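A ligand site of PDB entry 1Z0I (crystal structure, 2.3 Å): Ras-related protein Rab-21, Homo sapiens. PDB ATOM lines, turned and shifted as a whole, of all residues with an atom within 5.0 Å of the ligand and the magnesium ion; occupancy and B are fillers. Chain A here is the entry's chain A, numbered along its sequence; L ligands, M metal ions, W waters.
N of Gly 18 lies within hydrogen-bond range of O4 of the ligand (3.0 Å). The side-chain amino group (NZ) of Lys 19 lies within salt-bridge range of an oxygen (O2) of the ligand (2.6 Å). OD2 of Asp 122 sits at hydrogen-bond distance from N4 of the ligand, 2.9 Å away. O of Asn 32 lies within hydrogen-bond range of O10 of the ligand (2.8 Å). An oxygen (O5) of the ligand lies within hydrogen-bond range of the backbone NH of Ser 21, at 2.9 Å. OG of Ser 21 lies within hydrogen-bond range of O5 of the ligand. The backbone NH (N) of Thr 20 sits close to an oxygen (O3) of the ligand, at 3.0 Å. O9 of the ligand lies within hydrogen-bond range of OD2 of Asp 33. An oxygen (O1) of the ligand lies within hydrogen-bond range of the backbone NH of Cys 16, 2.9 Å away. The backbone NH (N) of Lys 151 sits at hydrogen-bond distance from an oxygen (O11) of the ligand, 3.5 Å away. N of Ala 150 is in hydrogen-bond range of O11 of the ligand, at 2.9 Å. ND2 of Asn 119 is in hydrogen-bond range of N2 of the ligand (3.2 Å). N of Lys 19 sits at hydrogen-bond distance from O2 of the ligand (2.9 Å). An oxygen (O8) of the ligand sits at hydrogen-bond distance from the side-chain amino group (NZ) of Lys 120.
N of Ala 150 sits at hydrogen-bond distance from OD1 of Asn 119 (3.4 Å). The side-chain hydroxyl of Thr 148 is in hydrogen-bond range of the side-chain amide oxygen of Asn 119. The backbone NH of Lys 120 sits at hydrogen-bond distance from the backbone carbonyl oxygen of Thr 148 (2.8 Å). O of Cys 16 sits at hydrogen-bond distance from NZ of Lys 120 (2.9 Å). OG1 of Thr 20 lies close to OD1 of Asp 61 (2.7 Å). O of Val 17 lies within hydrogen-bond range of ND2 of Asn 119. OD1 of Asp 122 is in hydrogen-bond range of OG of Ser 149, at 2.9 Å. The backbone carbonyl oxygen of Glu 14 is in hydrogen-bond range of the side-chain amino group of Lys 19.
Glu 14 touches the ligand (O to O2, 3.9 Å). Gly 15 touches the ligand (CA to O1, 3.7 Å). Val 17 touches the ligand (N to O2, 3.5 Å). CE1 of Phe 31 touches O10 of the ligand (3.6 Å). Leu 123 touches the ligand (CD1 to N4, 3.7 Å). CA of Ser 149 touches O11 of the ligand, 3.5 Å away. Hydrophobic or aromatic side chains within 4 Å of the ligand: Val 17, Phe 31, Leu 123 and Ala 150. Along chain A the residues within 4 Å of the ligand span positions 14 to 151. The nearest printed residue that does not touch the ligand is Thr 37 (4.3 Å).
Within 4 Å of the magnesium ion: Thr 20. The nearest printed residue that does not touch the magnesium ion is Asp 61 (4.01 Å).
The magnesium ion is bound by water W5 (1.9 Å), OG1 of Thr 20 (2.1 Å), water W6 (2.2 Å), O3 of the ligand (2.3 Å), water W4 (2.4 Å) and water W3 (2.5 Å). The magnesium ion has six donor atoms within binding distance.
Water W4 lies within hydrogen-bond range of O of Thr 37 and O6 of the ligand. Water W6 lies within hydrogen-bond range of O of Thr 62 (2.6 Å) and OD2 of Asp 61 (2.7 Å). Water W7 bridges the side-chain amino group (NZ) of Lys 120 (3.1 Å) and a nitrogen (N5) of the ligand (3.1 Å). Water W1 lies within hydrogen-bond range of O6 of the ligand (3.1 Å) and N of Thr 37 (3.2 Å). Water W8 lies within hydrogen-bond range of OG1 of Thr 37, O of Asn 32, OG of Ser 21 and O10 of the ligand.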
ATOM      1  N   GLU A  14     -10.768  29.005  -7.327  1.00  0.00           N
ATOM      2  CA  GLU A  14      -9.659  29.584  -8.094  1.00  0.00           C
ATOM      3  C   GLU A  14      -9.297  28.729  -9.319  1.00  0.00           C
ATOM      4  O   GLU A  14      -9.576  27.522  -9.329  1.00  0.00           O
ATOM      5  CB  GLU A  14      -8.409  29.794  -7.226  1.00  0.00           C
ATOM      6  CG  GLU A  14      -8.633  30.711  -6.049  1.00  0.00           C
ATOM      7  CD  GLU A  14      -9.159  32.072  -6.466  1.00  0.00           C
ATOM      8  OE1 GLU A  14      -8.389  32.828  -7.125  1.00  0.00           O
ATOM      9  OE2 GLU A  14     -10.321  32.393  -6.136  1.00  0.00           O
ATOM     10  N   GLY A  15      -8.682  29.356 -10.318  1.00  0.00           N
ATOM     11  CA  GLY A  15      -8.143  28.649 -11.488  1.00  0.00           C
ATOM     12  C   GLY A  15      -7.057  27.650 -11.127  1.00  0.00           C
ATOM     13  O   GLY A  15      -6.281  27.860 -10.184  1.00  0.00           O
ATOM     14  N   CYS A  16      -7.006  26.568 -11.906  1.00  0.00           N
ATOM     15  CA  CYS A  16      -6.052  25.446 -11.761  1.00  0.00           C
ATOM     16  C   CYS A  16      -6.409  24.373 -10.708  1.00  0.00           C
ATOM     17  O   CYS A  16      -5.710  23.359 -10.601  1.00  0.00           O
ATOM     18  CB  CYS A  16      -4.620  25.924 -11.557  1.00  0.00           C
ATOM     19  SG  CYS A  16      -4.063  27.150 -12.725  1.00  0.00           S
ATOM     20  N   VAL A  17      -7.487  24.571  -9.950  1.00  0.00           N
ATOM     21  CA  VAL A  17      -7.844  23.595  -8.901  1.00  0.00           C
ATOM     22  C   VAL A  17      -8.494  22.260  -9.380  1.00  0.00           C
ATOM     23  O   VAL A  17      -8.511  21.261  -8.632  1.00  0.00           O
ATOM     24  CB  VAL A  17      -8.665  24.242  -7.747  1.00  0.00           C
ATOM     25  CG1 VAL A  17      -7.953  25.461  -7.182  1.00  0.00           C
ATOM     26  CG2 VAL A  17     -10.068  24.600  -8.204  1.00  0.00           C
ATOM     27  N   GLY A  18      -9.023  22.242 -10.595  1.00  0.00           N
ATOM     28  CA  GLY A  18      -9.652  21.039 -11.149  1.00  0.00           C
ATOM     29  C   GLY A  18     -11.158  21.079 -11.398  1.00  0.00           C
ATOM     30  O   GLY A  18     -11.777  20.036 -11.621  1.00  0.00           O
ATOM     31  N   LYS A  19     -11.739  22.286 -11.396  1.00  0.00           N
ATOM     32  CA  LYS A  19     -13.188  22.438 -11.628  1.00  0.00           C
ATOM     33  C   LYS A  19     -13.649  21.796 -12.938  1.00  0.00           C
ATOM     34  O   LYS A  19     -14.603  21.007 -12.942  1.00  0.00           O
ATOM     35  CB  LYS A  19     -13.603  23.928 -11.581  1.00  0.00           C
ATOM     36  CG  LYS A  19     -13.258  24.655 -10.273  1.00  0.00           C
ATOM     37  CD  LYS A  19     -13.860  26.063 -10.202  1.00  0.00           C
ATOM     38  CE  LYS A  19     -13.252  27.074 -11.222  1.00  0.00           C
ATOM     39  NZ  LYS A  19     -11.807  26.882 -11.472  1.00  0.00           N
ATOM     40  N   THR A  20     -12.984  22.109 -14.051  1.00  0.00           N
ATOM     41  CA  THR A  20     -13.369  21.533 -15.365  1.00  0.00           C
ATOM     42  C   THR A  20     -13.077  20.036 -15.452  1.00  0.00           C
ATOM     43  O   THR A  20     -13.841  19.299 -16.092  1.00  0.00           O
ATOM     44  CB  THR A  20     -12.678  22.239 -16.562  1.00  0.00           C
ATOM     45  OG1 THR A  20     -12.808  23.663 -16.419  1.00  0.00           O
ATOM     46  CG2 THR A  20     -13.307  21.816 -17.893  1.00  0.00           C
ATOM     47  N   SER A  21     -11.987  19.578 -14.827  1.00  0.00           N
ATOM     48  CA  SER A  21     -11.641  18.154 -14.843  1.00  0.00           C
ATOM     49  C   SER A  21     -12.717  17.333 -14.160  1.00  0.00           C
ATOM     50  O   SER A  21     -13.051  16.234 -14.623  1.00  0.00           O
ATOM     51  CB  SER A  21     -10.287  17.885 -14.211  1.00  0.00           C
ATOM     52  OG  SER A  21      -9.303  18.727 -14.780  1.00  0.00           O
ATOM     53  N   PHE A  31     -10.149  12.208 -18.664  1.00  0.00           N
ATOM     54  CA  PHE A  31      -9.183  12.999 -17.907  1.00  0.00           C
ATOM     55  C   PHE A  31      -7.878  13.124 -18.682  1.00  0.00           C
ATOM     56  O   PHE A  31      -7.329  12.116 -19.170  1.00  0.00           O
ATOM     57  CB  PHE A  31      -8.890  12.412 -16.519  1.00  0.00           C
ATOM     58  CG  PHE A  31      -7.753  13.107 -15.803  1.00  0.00           C
ATOM     59  CD1 PHE A  31      -7.993  14.233 -15.027  1.00  0.00           C
ATOM     60  CD2 PHE A  31      -6.447  12.632 -15.932  1.00  0.00           C
ATOM     61  CE1 PHE A  31      -6.935  14.907 -14.381  1.00  0.00           C
ATOM     62  CE2 PHE A  31      -5.383  13.286 -15.293  1.00  0.00           C
ATOM     63  CZ  PHE A  31      -5.621  14.426 -14.513  1.00  0.00           C
ATOM     64  N   ASN A  32      -7.375  14.350 -18.759  1.00  0.00           N
ATOM     65  CA  ASN A  32      -6.124  14.626 -19.437  1.00  0.00           C
ATOM     66  C   ASN A  32      -5.264  15.660 -18.691  1.00  0.00           C
ATOM     67  O   ASN A  32      -5.784  16.696 -18.248  1.00  0.00           O
ATOM     68  CB  ASN A  32      -6.420  15.091 -20.862  1.00  0.00           C
ATOM     69  CG  ASN A  32      -5.175  15.372 -21.656  1.00  0.00           C
ATOM     70  OD1 ASN A  32      -4.726  14.544 -22.462  1.00  0.00           O
ATOM     71  ND2 ASN A  32      -4.584  16.541 -21.429  1.00  0.00           N
ATOM     72  N   ASP A  33      -3.963  15.372 -18.530  1.00  0.00           N
ATOM     73  CA  ASP A  33      -3.027  16.318 -17.892  1.00  0.00           C
ATOM     74  C   ASP A  33      -1.912  16.781 -18.861  1.00  0.00           C
ATOM     75  O   ASP A  33      -0.811  17.107 -18.435  1.00  0.00           O
ATOM     76  CB  ASP A  33      -2.468  15.750 -16.572  1.00  0.00           C
ATOM     77  CG  ASP A  33      -1.698  16.802 -15.726  1.00  0.00           C
ATOM     78  OD1 ASP A  33      -0.730  16.436 -15.023  1.00  0.00           O
ATOM     79  OD2 ASP A  33      -2.038  18.011 -15.757  1.00  0.00           O
ATOM     80  N   THR A  37      -7.662  21.958 -20.679  1.00  0.00           N
ATOM     81  CA  THR A  37      -9.047  21.492 -20.850  1.00  0.00           C
ATOM     82  C   THR A  37     -10.032  22.644 -20.724  1.00  0.00           C
ATOM     83  O   THR A  37      -9.902  23.496 -19.834  1.00  0.00           O
ATOM     84  CB  THR A  37      -9.484  20.413 -19.817  1.00  0.00           C
ATOM     85  OG1 THR A  37      -8.368  19.608 -19.417  1.00  0.00           O
ATOM     86  CG2 THR A  37     -10.529  19.516 -20.438  1.00  0.00           C
ATOM     87  N   ASP A  61     -19.966  25.292 -15.642  1.00  0.00           N
ATOM     88  CA  ASP A  61     -18.540  25.566 -15.446  1.00  0.00           C
ATOM     89  C   ASP A  61     -18.187  26.880 -16.148  1.00  0.00           C
ATOM     90  O   ASP A  61     -18.835  27.257 -17.115  1.00  0.00           O
ATOM     91  CB  ASP A  61     -17.712  24.384 -16.001  1.00  0.00           C
ATOM     92  CG  ASP A  61     -16.208  24.527 -15.771  1.00  0.00           C
ATOM     93  OD1 ASP A  61     -15.455  24.184 -16.700  1.00  0.00           O
ATOM     94  OD2 ASP A  61     -15.778  24.962 -14.680  1.00  0.00           O
ATOM     95  N   THR A  62     -17.189  27.585 -15.648  1.00  0.00           N
ATOM     96  CA  THR A  62     -16.678  28.816 -16.307  1.00  0.00           C
ATOM     97  C   THR A  62     -15.154  28.856 -16.400  1.00  0.00           C
ATOM     98  O   THR A  62     -14.461  28.505 -15.450  1.00  0.00           O
ATOM     99  CB  THR A  62     -17.210  30.115 -15.635  1.00  0.00           C
ATOM    100  OG1 THR A  62     -16.865  31.242 -16.448  1.00  0.00           O
ATOM    101  CG2 THR A  62     -16.650  30.327 -14.205  1.00  0.00           C
ATOM    102  N   ALA A  63     -14.649  29.296 -17.554  1.00  0.00           N
ATOM    103  CA  ALA A  63     -13.201  29.395 -17.835  1.00  0.00           C
ATOM    104  C   ALA A  63     -12.446  30.531 -17.145  1.00  0.00           C
ATOM    105  O   ALA A  63     -13.054  31.443 -16.579  1.00  0.00           O
ATOM    106  CB  ALA A  63     -12.953  29.457 -19.351  1.00  0.00           C
ATOM    107  N   ASN A 119      -9.751  18.780  -3.922  1.00  0.00           N
ATOM    108  CA  ASN A 119      -9.373  17.951  -5.089  1.00  0.00           C
ATOM    109  C   ASN A 119      -7.878  17.655  -5.168  1.00  0.00           C
ATOM    110  O   ASN A 119      -7.071  18.406  -4.603  1.00  0.00           O
ATOM    111  CB  ASN A 119      -9.867  18.567  -6.404  1.00  0.00           C
ATOM    112  CG  ASN A 119      -9.693  17.629  -7.604  1.00  0.00           C
ATOM    113  OD1 ASN A 119     -10.119  16.467  -7.576  1.00  0.00           O
ATOM    114  ND2 ASN A 119      -9.059  18.126  -8.661  1.00  0.00           N
ATOM    115  N   LYS A 120      -7.517  16.578  -5.901  1.00  0.00           N
ATOM    116  CA  LYS A 120      -6.131  16.193  -6.214  1.00  0.00           C
ATOM    117  C   LYS A 120      -5.490  15.336  -5.120  1.00  0.00           C
ATOM    118  O   LYS A 120      -4.289  15.466  -4.818  1.00  0.00           O
ATOM    119  CB  LYS A 120      -5.237  17.429  -6.512  1.00  0.00           C
ATOM    120  CG  LYS A 120      -5.583  18.167  -7.804  1.00  0.00           C
ATOM    121  CD  LYS A 120      -4.530  19.206  -8.203  1.00  0.00           C
ATOM    122  CE  LYS A 120      -5.079  20.058  -9.362  1.00  0.00           C
ATOM    123  NZ  LYS A 120      -4.124  21.039  -9.923  1.00  0.00           N
ATOM    124  N   ILE A 121      -6.280  14.431  -4.533  1.00  0.00           N
ATOM    125  CA  ILE A 121      -5.804  13.692  -3.349  1.00  0.00           C
ATOM    126  C   ILE A 121      -4.798  12.575  -3.668  1.00  0.00           C
ATOM    127  O   ILE A 121      -4.206  11.988  -2.758  1.00  0.00           O
ATOM    128  CB  ILE A 121      -6.962  13.160  -2.463  1.00  0.00           C
ATOM    129  CG1 ILE A 121      -7.862  12.207  -3.280  1.00  0.00           C
ATOM    130  CG2 ILE A 121      -7.696  14.348  -1.794  1.00  0.00           C
ATOM    131  CD1 ILE A 121      -8.844  11.377  -2.455  1.00  0.00           C
ATOM    132  N   ASP A 122      -4.618  12.286  -4.965  1.00  0.00           N
ATOM    133  CA  ASP A 122      -3.533  11.426  -5.437  1.00  0.00           C
ATOM    134  C   ASP A 122      -2.156  12.040  -5.141  1.00  0.00           C
ATOM    135  O   ASP A 122      -1.140  11.333  -5.128  1.00  0.00           O
ATOM    136  CB  ASP A 122      -3.666  11.161  -6.955  1.00  0.00           C
ATOM    137  CG  ASP A 122      -3.761  12.451  -7.773  1.00  0.00           C
ATOM    138  OD1 ASP A 122      -4.738  13.234  -7.622  1.00  0.00           O
ATOM    139  OD2 ASP A 122      -2.834  12.679  -8.580  1.00  0.00           O
ATOM    140  N   LEU A 123      -2.129  13.354  -4.918  1.00  0.00           N
ATOM    141  CA  LEU A 123      -0.877  14.075  -4.647  1.00  0.00           C
ATOM    142  C   LEU A 123      -0.664  14.331  -3.158  1.00  0.00           C
ATOM    143  O   LEU A 123       0.008  15.296  -2.801  1.00  0.00           O
ATOM    144  CB  LEU A 123      -0.828  15.393  -5.426  1.00  0.00           C
ATOM    145  CG  LEU A 123      -0.891  15.367  -6.958  1.00  0.00           C
ATOM    146  CD1 LEU A 123      -0.999  16.782  -7.504  1.00  0.00           C
ATOM    147  CD2 LEU A 123       0.297  14.602  -7.610  1.00  0.00           C
ATOM    148  N   THR A 148     -11.701  14.528  -3.332  1.00  0.00           N
ATOM    149  CA  THR A 148     -11.769  13.991  -4.714  1.00  0.00           C
ATOM    150  C   THR A 148     -10.422  13.894  -5.417  1.00  0.00           C
ATOM    151  O   THR A 148      -9.520  14.691  -5.187  1.00  0.00           O
ATOM    152  CB  THR A 148     -12.632  14.869  -5.654  1.00  0.00           C
ATOM    153  OG1 THR A 148     -12.165  16.228  -5.580  1.00  0.00           O
ATOM    154  CG2 THR A 148     -14.101  14.778  -5.321  1.00  0.00           C
ATOM    155  N   SER A 149     -10.302  12.939  -6.332  1.00  0.00           N
ATOM    156  CA  SER A 149      -9.210  12.922  -7.301  1.00  0.00           C
ATOM    157  C   SER A 149      -9.822  12.663  -8.663  1.00  0.00           C
ATOM    158  O   SER A 149     -10.345  11.581  -8.918  1.00  0.00           O
ATOM    159  CB  SER A 149      -8.174  11.846  -6.949  1.00  0.00           C
ATOM    160  OG  SER A 149      -7.184  11.747  -7.976  1.00  0.00           O
ATOM    161  N   ALA A 150      -9.776  13.676  -9.536  1.00  0.00           N
ATOM    162  CA  ALA A 150     -10.261  13.559 -10.917  1.00  0.00           C
ATOM    163  C   ALA A 150      -9.352  12.660 -11.782  1.00  0.00           C
ATOM    164  O   ALA A 150      -9.803  12.051 -12.757  1.00  0.00           O
ATOM    165  CB  ALA A 150     -10.392  14.939 -11.542  1.00  0.00           C
ATOM    166  N   LYS A 151      -8.074  12.605 -11.410  1.00  0.00           N
ATOM    167  CA  LYS A 151      -7.051  11.860 -12.112  1.00  0.00           C
ATOM    168  C   LYS A 151      -7.266  10.355 -11.995  1.00  0.00           C
ATOM    169  O   LYS A 151      -7.150   9.640 -12.998  1.00  0.00           O
ATOM    170  CB  LYS A 151      -5.646  12.240 -11.602  1.00  0.00           C
ATOM    171  CG  LYS A 151      -4.528  11.459 -12.291  1.00  0.00           C
ATOM    172  CD  LYS A 151      -3.130  11.969 -11.946  1.00  0.00           C
ATOM    173  CE  LYS A 151      -2.100  11.023 -12.592  1.00  0.00           C
ATOM    174  NZ  LYS A 151      -0.706  11.315 -12.160  1.00  0.00           N
HETATM  175  P1  LIG L   1      -9.814  24.594 -13.357  1.00  0.00           P
HETATM  176  O1  LIG L   1      -9.075  25.869 -13.747  1.00  0.00           O
HETATM  177  O2  LIG L   1     -10.357  24.803 -11.979  1.00  0.00           O
HETATM  178  O3  LIG L   1     -10.929  24.309 -14.336  1.00  0.00           O
HETATM  179  O4  LIG L   1      -8.722  23.380 -13.361  1.00  0.00           O
HETATM  180  P2  LIG L   1      -8.499  22.324 -14.570  1.00  0.00           P
HETATM  181  O5  LIG L   1      -9.604  21.278 -14.660  1.00  0.00           O
HETATM  182  O6  LIG L   1      -8.305  22.928 -15.913  1.00  0.00           O
HETATM  183  O7  LIG L   1      -7.159  21.553 -14.133  1.00  0.00           O
HETATM  184  C1  LIG L   1      -5.887  22.172 -13.988  1.00  0.00           C
HETATM  185  C2  LIG L   1      -4.798  21.100 -14.122  1.00  0.00           C
HETATM  186  O8  LIG L   1      -4.747  20.202 -13.005  1.00  0.00           O
HETATM  187  C3  LIG L   1      -4.968  20.231 -15.345  1.00  0.00           C
HETATM  188  O9  LIG L   1      -3.666  19.857 -15.736  1.00  0.00           O
HETATM  189  C4  LIG L   1      -5.617  18.966 -14.827  1.00  0.00           C
HETATM  190  O10 LIG L   1      -5.350  17.855 -15.706  1.00  0.00           O
HETATM  191  C5  LIG L   1      -4.958  18.858 -13.452  1.00  0.00           C
HETATM  192  N1  LIG L   1      -5.800  18.103 -12.496  1.00  0.00           N
HETATM  193  C6  LIG L   1      -7.128  18.251 -12.308  1.00  0.00           C
HETATM  194  N2  LIG L   1      -7.593  17.394 -11.373  1.00  0.00           N
HETATM  195  C7  LIG L   1      -6.545  16.697 -10.907  1.00  0.00           C
HETATM  196  C8  LIG L   1      -6.370  15.637  -9.901  1.00  0.00           C
HETATM  197  O11 LIG L   1      -7.337  15.197  -9.245  1.00  0.00           O
HETATM  198  N3  LIG L   1      -5.127  15.168  -9.723  1.00  0.00           N
HETATM  199  C9  LIG L   1      -4.058  15.606 -10.434  1.00  0.00           C
HETATM  200  N4  LIG L   1      -2.844  15.041 -10.177  1.00  0.00           N
HETATM  201  N5  LIG L   1      -4.148  16.584 -11.394  1.00  0.00           N
HETATM  202  C10 LIG L   1      -5.358  17.159 -11.660  1.00  0.00           C
HETATM  203 MG    MG M   1     -11.705  25.478 -16.134  1.00  0.00          MG
HETATM  204  O   HOH W   1      -6.128  23.081 -18.152  1.00  0.00           O
HETATM  205  O   HOH W   2      -2.627  23.423 -14.461  1.00  0.00           O
HETATM  206  O   HOH W   3     -10.132  27.324 -15.508  1.00  0.00           O
HETATM  207  O   HOH W   4     -10.054  24.289 -17.415  1.00  0.00           O
HETATM  208  O   HOH W   5     -12.159  26.305 -17.812  1.00  0.00           O
HETATM  209  O   HOH W   6     -13.423  26.201 -14.942  1.00  0.00           O
HETATM  210  O   HOH W   7      -2.231  19.017 -11.234  1.00  0.00           O
HETATM  211  O   HOH W   8      -7.999  18.249 -17.362  1.00  0.00           O
